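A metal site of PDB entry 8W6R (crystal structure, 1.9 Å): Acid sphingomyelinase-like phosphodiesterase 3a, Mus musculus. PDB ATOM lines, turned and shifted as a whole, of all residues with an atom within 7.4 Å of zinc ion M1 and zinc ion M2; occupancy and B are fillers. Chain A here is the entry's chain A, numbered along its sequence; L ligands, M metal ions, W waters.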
ATOM      1  N   THR A  19      30.558  22.273 -16.141  1.00  0.00           N
ATOM      2  CA  THR A  19      30.047  20.939 -15.848  1.00  0.00           C
ATOM      3  C   THR A  19      30.276  20.612 -14.379  1.00  0.00           C
ATOM      4  O   THR A  19      31.164  21.169 -13.727  1.00  0.00           O
ATOM      5  CB  THR A  19      30.727  19.865 -16.734  1.00  0.00           C
ATOM      6  OG1 THR A  19      30.033  18.623 -16.610  1.00  0.00           O
ATOM      7  CG2 THR A  19      32.172  19.635 -16.296  1.00  0.00           C
ATOM      8  N   ASP A  20      29.464  19.693 -13.879  1.00  0.00           N
ATOM      9  CA  ASP A  20      29.647  19.105 -12.549  1.00  0.00           C
ATOM     10  C   ASP A  20      29.743  20.191 -11.489  1.00  0.00           C
ATOM     11  O   ASP A  20      30.717  20.296 -10.740  1.00  0.00           O
ATOM     12  CB  ASP A  20      30.849  18.186 -12.506  1.00  0.00           C
ATOM     13  CG  ASP A  20      30.632  16.949 -13.362  1.00  0.00           C
ATOM     14  OD1 ASP A  20      30.044  15.984 -12.820  1.00  0.00           O
ATOM     15  OD2 ASP A  20      30.992  16.972 -14.570  1.00  0.00           O
ATOM     16  N   LEU A  21      28.690  21.006 -11.453  1.00  0.00           N
ATOM     17  CA  LEU A  21      28.595  22.115 -10.516  1.00  0.00           C
ATOM     18  C   LEU A  21      28.467  21.589  -9.088  1.00  0.00           C
ATOM     19  O   LEU A  21      29.131  22.093  -8.165  1.00  0.00           O
ATOM     20  CB  LEU A  21      27.401  22.976 -10.912  1.00  0.00           C
ATOM     21  CG  LEU A  21      27.511  23.702 -12.265  1.00  0.00           C
ATOM     22  CD1 LEU A  21      26.294  24.600 -12.521  1.00  0.00           C
ATOM     23  CD2 LEU A  21      28.788  24.500 -12.417  1.00  0.00           C
ATOM     24  N   HIS A  22      27.604  20.596  -8.877  1.00  0.00           N
ATOM     25  CA  HIS A  22      27.404  19.937  -7.576  1.00  0.00           C
ATOM     26  C   HIS A  22      27.262  20.923  -6.419  1.00  0.00           C
ATOM     27  O   HIS A  22      28.059  20.930  -5.468  1.00  0.00           O
ATOM     28  CB  HIS A  22      28.540  18.968  -7.266  1.00  0.00           C
ATOM     29  CG  HIS A  22      28.558  17.756  -8.139  1.00  0.00           C
ATOM     30  ND1 HIS A  22      27.612  16.758  -8.041  1.00  0.00           N
ATOM     31  CD2 HIS A  22      29.444  17.343  -9.075  1.00  0.00           C
ATOM     32  CE1 HIS A  22      27.897  15.799  -8.912  1.00  0.00           C
ATOM     33  NE2 HIS A  22      29.004  16.126  -9.540  1.00  0.00           N
ATOM     34  N   ASP A  57      31.437  19.357  -1.562  1.00  0.00           N
ATOM     35  CA  ASP A  57      30.936  19.868  -2.818  1.00  0.00           C
ATOM     36  C   ASP A  57      30.846  21.409  -2.758  1.00  0.00           C
ATOM     37  O   ASP A  57      31.209  22.034  -1.770  1.00  0.00           O
ATOM     38  CB  ASP A  57      29.584  19.242  -3.124  1.00  0.00           C
ATOM     39  CG  ASP A  57      29.710  18.002  -3.973  1.00  0.00           C
ATOM     40  OD1 ASP A  57      30.510  18.048  -4.925  1.00  0.00           O
ATOM     41  OD2 ASP A  57      29.050  16.982  -3.674  1.00  0.00           O
ATOM     42  N   THR A  83      27.133  20.332 -18.968  1.00  0.00           N
ATOM     43  CA  THR A  83      26.935  18.890 -19.081  1.00  0.00           C
ATOM     44  C   THR A  83      26.662  18.177 -17.758  1.00  0.00           C
ATOM     45  O   THR A  83      27.175  17.089 -17.523  1.00  0.00           O
ATOM     46  CB  THR A  83      28.131  18.265 -19.816  1.00  0.00           C
ATOM     47  OG1 THR A  83      29.355  18.579 -19.131  1.00  0.00           O
ATOM     48  CG2 THR A  83      28.216  18.795 -21.246  1.00  0.00           C
ATOM     49  N   GLY A  84      25.807  18.727 -16.884  1.00  0.00           N
ATOM     50  CA  GLY A  84      25.139  17.905 -15.885  1.00  0.00           C
ATOM     51  C   GLY A  84      25.776  17.876 -14.520  1.00  0.00           C
ATOM     52  O   GLY A  84      26.814  18.475 -14.260  1.00  0.00           O
ATOM     53  N   ASP A  85      25.151  17.078 -13.636  1.00  0.00           N
ATOM     54  CA  ASP A  85      25.449  16.910 -12.208  1.00  0.00           C
ATOM     55  C   ASP A  85      25.372  18.117 -11.297  1.00  0.00           C
ATOM     56  O   ASP A  85      26.380  18.612 -10.791  1.00  0.00           O
ATOM     57  CB  ASP A  85      26.809  16.259 -11.895  1.00  0.00           C
ATOM     58  CG  ASP A  85      26.847  14.750 -12.148  1.00  0.00           C
ATOM     59  OD1 ASP A  85      25.761  14.136 -12.090  1.00  0.00           O
ATOM     60  OD2 ASP A  85      27.949  14.137 -12.061  1.00  0.00           O
ATOM     61  N   SER A  86      24.155  18.505 -10.961  1.00  0.00           N
ATOM     62  CA  SER A  86      23.994  19.706 -10.150  1.00  0.00           C
ATOM     63  C   SER A  86      23.768  19.404  -8.671  1.00  0.00           C
ATOM     64  O   SER A  86      24.216  20.198  -7.843  1.00  0.00           O
ATOM     65  CB  SER A  86      22.861  20.554 -10.732  1.00  0.00           C
ATOM     66  OG  SER A  86      23.213  20.980 -12.039  1.00  0.00           O
ATOM     67  N   PRO A  87      23.094  18.315  -8.269  1.00  0.00           N
ATOM     68  CA  PRO A  87      22.956  18.034  -6.838  1.00  0.00           C
ATOM     69  C   PRO A  87      24.257  17.535  -6.245  1.00  0.00           C
ATOM     70  O   PRO A  87      25.154  17.071  -6.981  1.00  0.00           O
ATOM     71  CB  PRO A  87      21.871  16.932  -6.795  1.00  0.00           C
ATOM     72  CG  PRO A  87      21.116  17.119  -8.107  1.00  0.00           C
ATOM     73  CD  PRO A  87      22.259  17.376  -9.045  1.00  0.00           C
ATOM     74  N   HIS A  89      26.958  15.366  -3.545  1.00  0.00           N
ATOM     75  CA  HIS A  89      27.263  13.963  -3.245  1.00  0.00           C
ATOM     76  C   HIS A  89      26.840  13.721  -1.804  1.00  0.00           C
ATOM     77  O   HIS A  89      27.638  13.845  -0.877  1.00  0.00           O
ATOM     78  CB  HIS A  89      28.746  13.681  -3.424  1.00  0.00           C
ATOM     79  CG  HIS A  89      29.190  13.750  -4.848  1.00  0.00           C
ATOM     80  ND1 HIS A  89      29.598  14.922  -5.440  1.00  0.00           N
ATOM     81  CD2 HIS A  89      29.289  12.799  -5.809  1.00  0.00           C
ATOM     82  CE1 HIS A  89      29.932  14.684  -6.700  1.00  0.00           C
ATOM     83  NE2 HIS A  89      29.752  13.409  -6.942  1.00  0.00           N
ATOM     84  N   GLY A 125      23.185  14.805 -15.883  1.00  0.00           N
ATOM     85  CA  GLY A 125      24.211  13.989 -15.274  1.00  0.00           C
ATOM     86  C   GLY A 125      23.568  12.908 -14.424  1.00  0.00           C
ATOM     87  O   GLY A 125      22.374  12.927 -14.133  1.00  0.00           O
ATOM     88  N   ASN A 126      24.397  11.956 -13.980  1.00  0.00           N
ATOM     89  CA  ASN A 126      23.834  10.831 -13.239  1.00  0.00           C
ATOM     90  C   ASN A 126      23.254  11.267 -11.906  1.00  0.00           C
ATOM     91  O   ASN A 126      22.352  10.588 -11.387  1.00  0.00           O
ATOM     92  CB  ASN A 126      24.878   9.716 -13.066  1.00  0.00           C
ATOM     93  CG  ASN A 126      26.181  10.235 -12.443  1.00  0.00           C
ATOM     94  OD1 ASN A 126      26.872  11.049 -13.040  1.00  0.00           O
ATOM     95  ND2 ASN A 126      26.516   9.731 -11.255  1.00  0.00           N
ATOM     96  N   HIS A 127      23.717  12.389 -11.333  1.00  0.00           N
ATOM     97  CA  HIS A 127      23.104  12.878 -10.101  1.00  0.00           C
ATOM     98  C   HIS A 127      21.844  13.707 -10.349  1.00  0.00           C
ATOM     99  O   HIS A 127      21.155  14.073  -9.386  1.00  0.00           O
ATOM    100  CB  HIS A 127      24.107  13.703  -9.289  1.00  0.00           C
ATOM    101  CG  HIS A 127      25.183  12.881  -8.671  1.00  0.00           C
ATOM    102  ND1 HIS A 127      25.162  12.489  -7.344  1.00  0.00           N
ATOM    103  CD2 HIS A 127      26.324  12.379  -9.196  1.00  0.00           C
ATOM    104  CE1 HIS A 127      26.248  11.777  -7.088  1.00  0.00           C
ATOM    105  NE2 HIS A 127      26.963  11.693  -8.197  1.00  0.00           N
ATOM    106  N   ASP A 133      21.678   8.042 -10.478  1.00  0.00           N
ATOM    107  CA  ASP A 133      22.081   7.012 -11.439  1.00  0.00           C
ATOM    108  C   ASP A 133      20.899   6.289 -12.080  1.00  0.00           C
ATOM    109  O   ASP A 133      21.077   5.668 -13.125  1.00  0.00           O
ATOM    110  CB  ASP A 133      23.007   5.965 -10.818  1.00  0.00           C
ATOM    111  CG  ASP A 133      24.196   6.586 -10.106  1.00  0.00           C
ATOM    112  OD1 ASP A 133      24.570   7.732 -10.432  1.00  0.00           O
ATOM    113  OD2 ASP A 133      24.777   5.881  -9.243  1.00  0.00           O
ATOM    114  N   ASN A 186      23.832   8.650 -19.291  1.00  0.00           N
ATOM    115  CA  ASN A 186      23.580   7.979 -18.025  1.00  0.00           C
ATOM    116  C   ASN A 186      22.759   6.720 -18.242  1.00  0.00           C
ATOM    117  O   ASN A 186      22.757   5.831 -17.383  1.00  0.00           O
ATOM    118  CB  ASN A 186      22.853   8.924 -17.078  1.00  0.00           C
ATOM    119  CG  ASN A 186      23.510  10.274 -17.007  1.00  0.00           C
ATOM    120  OD1 ASN A 186      24.611  10.420 -16.473  1.00  0.00           O
ATOM    121  ND2 ASN A 186      22.859  11.273 -17.589  1.00  0.00           N
ATOM    122  N   TYR A 189      25.369   4.102 -18.199  1.00  0.00           N
ATOM    123  CA  TYR A 189      26.293   4.109 -17.067  1.00  0.00           C
ATOM    124  C   TYR A 189      26.087   2.865 -16.215  1.00  0.00           C
ATOM    125  O   TYR A 189      24.953   2.511 -15.895  1.00  0.00           O
ATOM    126  CB  TYR A 189      26.018   5.378 -16.274  1.00  0.00           C
ATOM    127  CG  TYR A 189      26.900   5.679 -15.097  1.00  0.00           C
ATOM    128  CD1 TYR A 189      28.271   5.590 -15.172  1.00  0.00           C
ATOM    129  CD2 TYR A 189      26.332   6.107 -13.893  1.00  0.00           C
ATOM    130  CE1 TYR A 189      29.067   5.880 -14.067  1.00  0.00           C
ATOM    131  CE2 TYR A 189      27.115   6.408 -12.802  1.00  0.00           C
ATOM    132  CZ  TYR A 189      28.468   6.297 -12.889  1.00  0.00           C
ATOM    133  OH  TYR A 189      29.226   6.601 -11.777  1.00  0.00           O
ATOM    134  N   HIS A 227      27.013  13.829 -20.445  1.00  0.00           N
ATOM    135  CA  HIS A 227      27.688  13.828 -19.151  1.00  0.00           C
ATOM    136  C   HIS A 227      28.794  12.773 -19.108  1.00  0.00           C
ATOM    137  O   HIS A 227      29.986  13.090 -19.136  1.00  0.00           O
ATOM    138  CB  HIS A 227      26.678  13.583 -18.037  1.00  0.00           C
ATOM    139  CG  HIS A 227      27.277  13.682 -16.675  1.00  0.00           C
ATOM    140  ND1 HIS A 227      27.867  14.839 -16.209  1.00  0.00           N
ATOM    141  CD2 HIS A 227      27.388  12.769 -15.690  1.00  0.00           C
ATOM    142  CE1 HIS A 227      28.302  14.639 -14.978  1.00  0.00           C
ATOM    143  NE2 HIS A 227      28.018  13.392 -14.641  1.00  0.00           N
ATOM    144  N   VAL A 228      28.401  11.499 -19.034  1.00  0.00           N
ATOM    145  CA  VAL A 228      29.405  10.437 -18.970  1.00  0.00           C
ATOM    146  C   VAL A 228      30.026  10.268 -20.343  1.00  0.00           C
ATOM    147  O   VAL A 228      29.291  10.206 -21.349  1.00  0.00           O
ATOM    148  CB  VAL A 228      28.771   9.146 -18.477  1.00  0.00           C
ATOM    149  CG1 VAL A 228      29.871   8.088 -18.284  1.00  0.00           C
ATOM    150  CG2 VAL A 228      28.003   9.423 -17.211  1.00  0.00           C
ATOM    151  N   GLY A 267      31.606  15.656 -19.434  1.00  0.00           N
ATOM    152  CA  GLY A 267      32.033  15.902 -18.052  1.00  0.00           C
ATOM    153  C   GLY A 267      32.208  14.616 -17.239  1.00  0.00           C
ATOM    154  O   GLY A 267      32.875  13.686 -17.685  1.00  0.00           O
ATOM    155  N   HIS A 268      31.642  14.584 -16.039  1.00  0.00           N
ATOM    156  CA  HIS A 268      31.519  13.412 -15.177  1.00  0.00           C
ATOM    157  C   HIS A 268      32.817  12.991 -14.500  1.00  0.00           C
ATOM    158  O   HIS A 268      32.791  12.622 -13.327  1.00  0.00           O
ATOM    159  CB  HIS A 268      30.954  12.203 -15.944  1.00  0.00           C
ATOM    160  CG  HIS A 268      30.918  10.938 -15.134  1.00  0.00           C
ATOM    161  ND1 HIS A 268      29.986  10.721 -14.125  1.00  0.00           N
ATOM    162  CD2 HIS A 268      31.702   9.829 -15.171  1.00  0.00           C
ATOM    163  CE1 HIS A 268      30.213   9.535 -13.579  1.00  0.00           C
ATOM    164  NE2 HIS A 268      31.248   8.981 -14.198  1.00  0.00           N
ATOM    165  N   THR A 269      33.938  12.984 -15.203  1.00  0.00           N
ATOM    166  CA  THR A 269      35.144  12.500 -14.529  1.00  0.00           C
ATOM    167  C   THR A 269      35.775  13.529 -13.600  1.00  0.00           C
ATOM    168  O   THR A 269      36.642  13.151 -12.801  1.00  0.00           O
ATOM    169  CB  THR A 269      36.209  12.019 -15.528  1.00  0.00           C
ATOM    170  OG1 THR A 269      36.827  13.145 -16.158  1.00  0.00           O
ATOM    171  CG2 THR A 269      35.639  11.049 -16.587  1.00  0.00           C
ATOM    172  N   HIS A 270      35.376  14.807 -13.704  1.00  0.00           N
ATOM    173  CA  HIS A 270      35.923  15.881 -12.874  1.00  0.00           C
ATOM    174  C   HIS A 270      37.403  16.084 -13.153  1.00  0.00           C
ATOM    175  O   HIS A 270      38.145  16.566 -12.286  1.00  0.00           O
ATOM    176  CB  HIS A 270      35.726  15.631 -11.377  1.00  0.00           C
ATOM    177  CG  HIS A 270      34.300  15.514 -10.944  1.00  0.00           C
ATOM    178  ND1 HIS A 270      33.932  15.594  -9.620  1.00  0.00           N
ATOM    179  CD2 HIS A 270      33.165  15.308 -11.649  1.00  0.00           C
ATOM    180  CE1 HIS A 270      32.610  15.463  -9.527  1.00  0.00           C
ATOM    181  NE2 HIS A 270      32.130  15.286 -10.744  1.00  0.00           N
ATOM    182  N   ALA A 293      35.554  19.597 -13.323  1.00  0.00           N
ATOM    183  CA  ALA A 293      34.394  20.028 -12.560  1.00  0.00           C
ATOM    184  C   ALA A 293      34.613  21.417 -11.952  1.00  0.00           C
ATOM    185  O   ALA A 293      35.748  21.867 -11.768  1.00  0.00           O
ATOM    186  CB  ALA A 293      34.091  19.026 -11.445  1.00  0.00           C
ATOM    187  N   THR A 295      33.125  21.645  -8.917  1.00  0.00           N
ATOM    188  CA  THR A 295      33.310  21.134  -7.560  1.00  0.00           C
ATOM    189  C   THR A 295      34.736  20.605  -7.381  1.00  0.00           C
ATOM    190  O   THR A 295      35.319  20.045  -8.311  1.00  0.00           O
ATOM    191  CB  THR A 295      32.293  20.029  -7.233  1.00  0.00           C
ATOM    192  OG1 THR A 295      32.462  19.626  -5.860  1.00  0.00           O
ATOM    193  CG2 THR A 295      32.491  18.814  -8.116  1.00  0.00           C
ATOM    194  N   VAL A 297      35.353  18.366  -4.893  1.00  0.00           N
ATOM    195  CA  VAL A 297      35.119  17.338  -3.878  1.00  0.00           C
ATOM    196  C   VAL A 297      35.967  16.098  -4.133  1.00  0.00           C
ATOM    197  O   VAL A 297      36.244  15.723  -5.282  1.00  0.00           O
ATOM    198  CB  VAL A 297      33.621  17.007  -3.851  1.00  0.00           C
ATOM    199  CG1 VAL A 297      33.210  16.201  -5.094  1.00  0.00           C
ATOM    200  CG2 VAL A 297      33.229  16.243  -2.573  1.00  0.00           C
HETATM  201  S1  LIG L   1      30.100  11.482  -9.892  1.00  0.00           S
HETATM  202  O1  LIG L   1      30.079  12.937  -9.669  1.00  0.00           O
HETATM  203  O2  LIG L   1      29.059  11.182 -10.893  1.00  0.00           O
HETATM  204  O3  LIG L   1      31.436  11.076 -10.331  1.00  0.00           O
HETATM  205  O4  LIG L   1      29.723  10.748  -8.666  1.00  0.00           O
HETATM  206 ZN    ZN M   1      28.653  12.189 -12.822  1.00  0.00          ZN
HETATM  207 ZN    ZN M   2      29.938  14.824 -11.100  1.00  0.00          ZN
HETATM  208  O   HOH W   1      30.485  13.128 -12.247  1.00  0.00           O
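Zinc ion M2 is bound by the side-chain carboxylate of Asp 20 (2.1 Å), water W1 (2.1 Å), a ring nitrogen (NE2) of His 22 (2.2 Å), a ring nitrogen (NE2) of His 270 (2.3 Å), the side-chain carboxylate of Asp 85 (2.3 Å) and an oxygen (O1) of the ligand (2.4 Å).
The nearest printed residue that does not touch zinc ion M1 is Asp 20 (4.04 Å).
Zinc ion M1 is bound by OD1 of Asn 126 (2.1 Å), water W1 (2.1 Å), OD2 of Asp 85 (2.2 Å), O2 of the ligand (2.2 Å), NE2 of His 227 (2.3 Å) and ND1 of His 268 (2.4 Å).
Of the 26 residues printed, 4 come within 4 Å of zinc ion M2.
The side-chain carboxylate (OD2) of Asp 20 lies within hydrogen-bond range of the backbone NH (N) of His 268 (2.9 Å). O of Asp 20 lies within hydrogen-bond range of N of Thr 295 (3.3 Å). The backbone carbonyl oxygen (O) of Gly 84 lies within hydrogen-bond range of the backbone NH (N) of Asp 20 (2.9 Å). OG1 of Thr 19 lies within hydrogen-bond range of OD2 of Asp 20 (2.8 Å). N of Asn 126 sits at hydrogen-bond distance from OD1 of Asn 186, 2.9 Å away. O of Asp 85 lies within hydrogen-bond range of N of Leu 21, 3.4 Å away. A ring nitrogen (ND1) of His 22 sits at hydrogen-bond distance from the backbone carbonyl oxygen (O) of Pro 87 (2.7 Å). A ring nitrogen (ND1) of His 227 is in hydrogen-bond range of the backbone carbonyl oxygen (O) of Thr 83.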
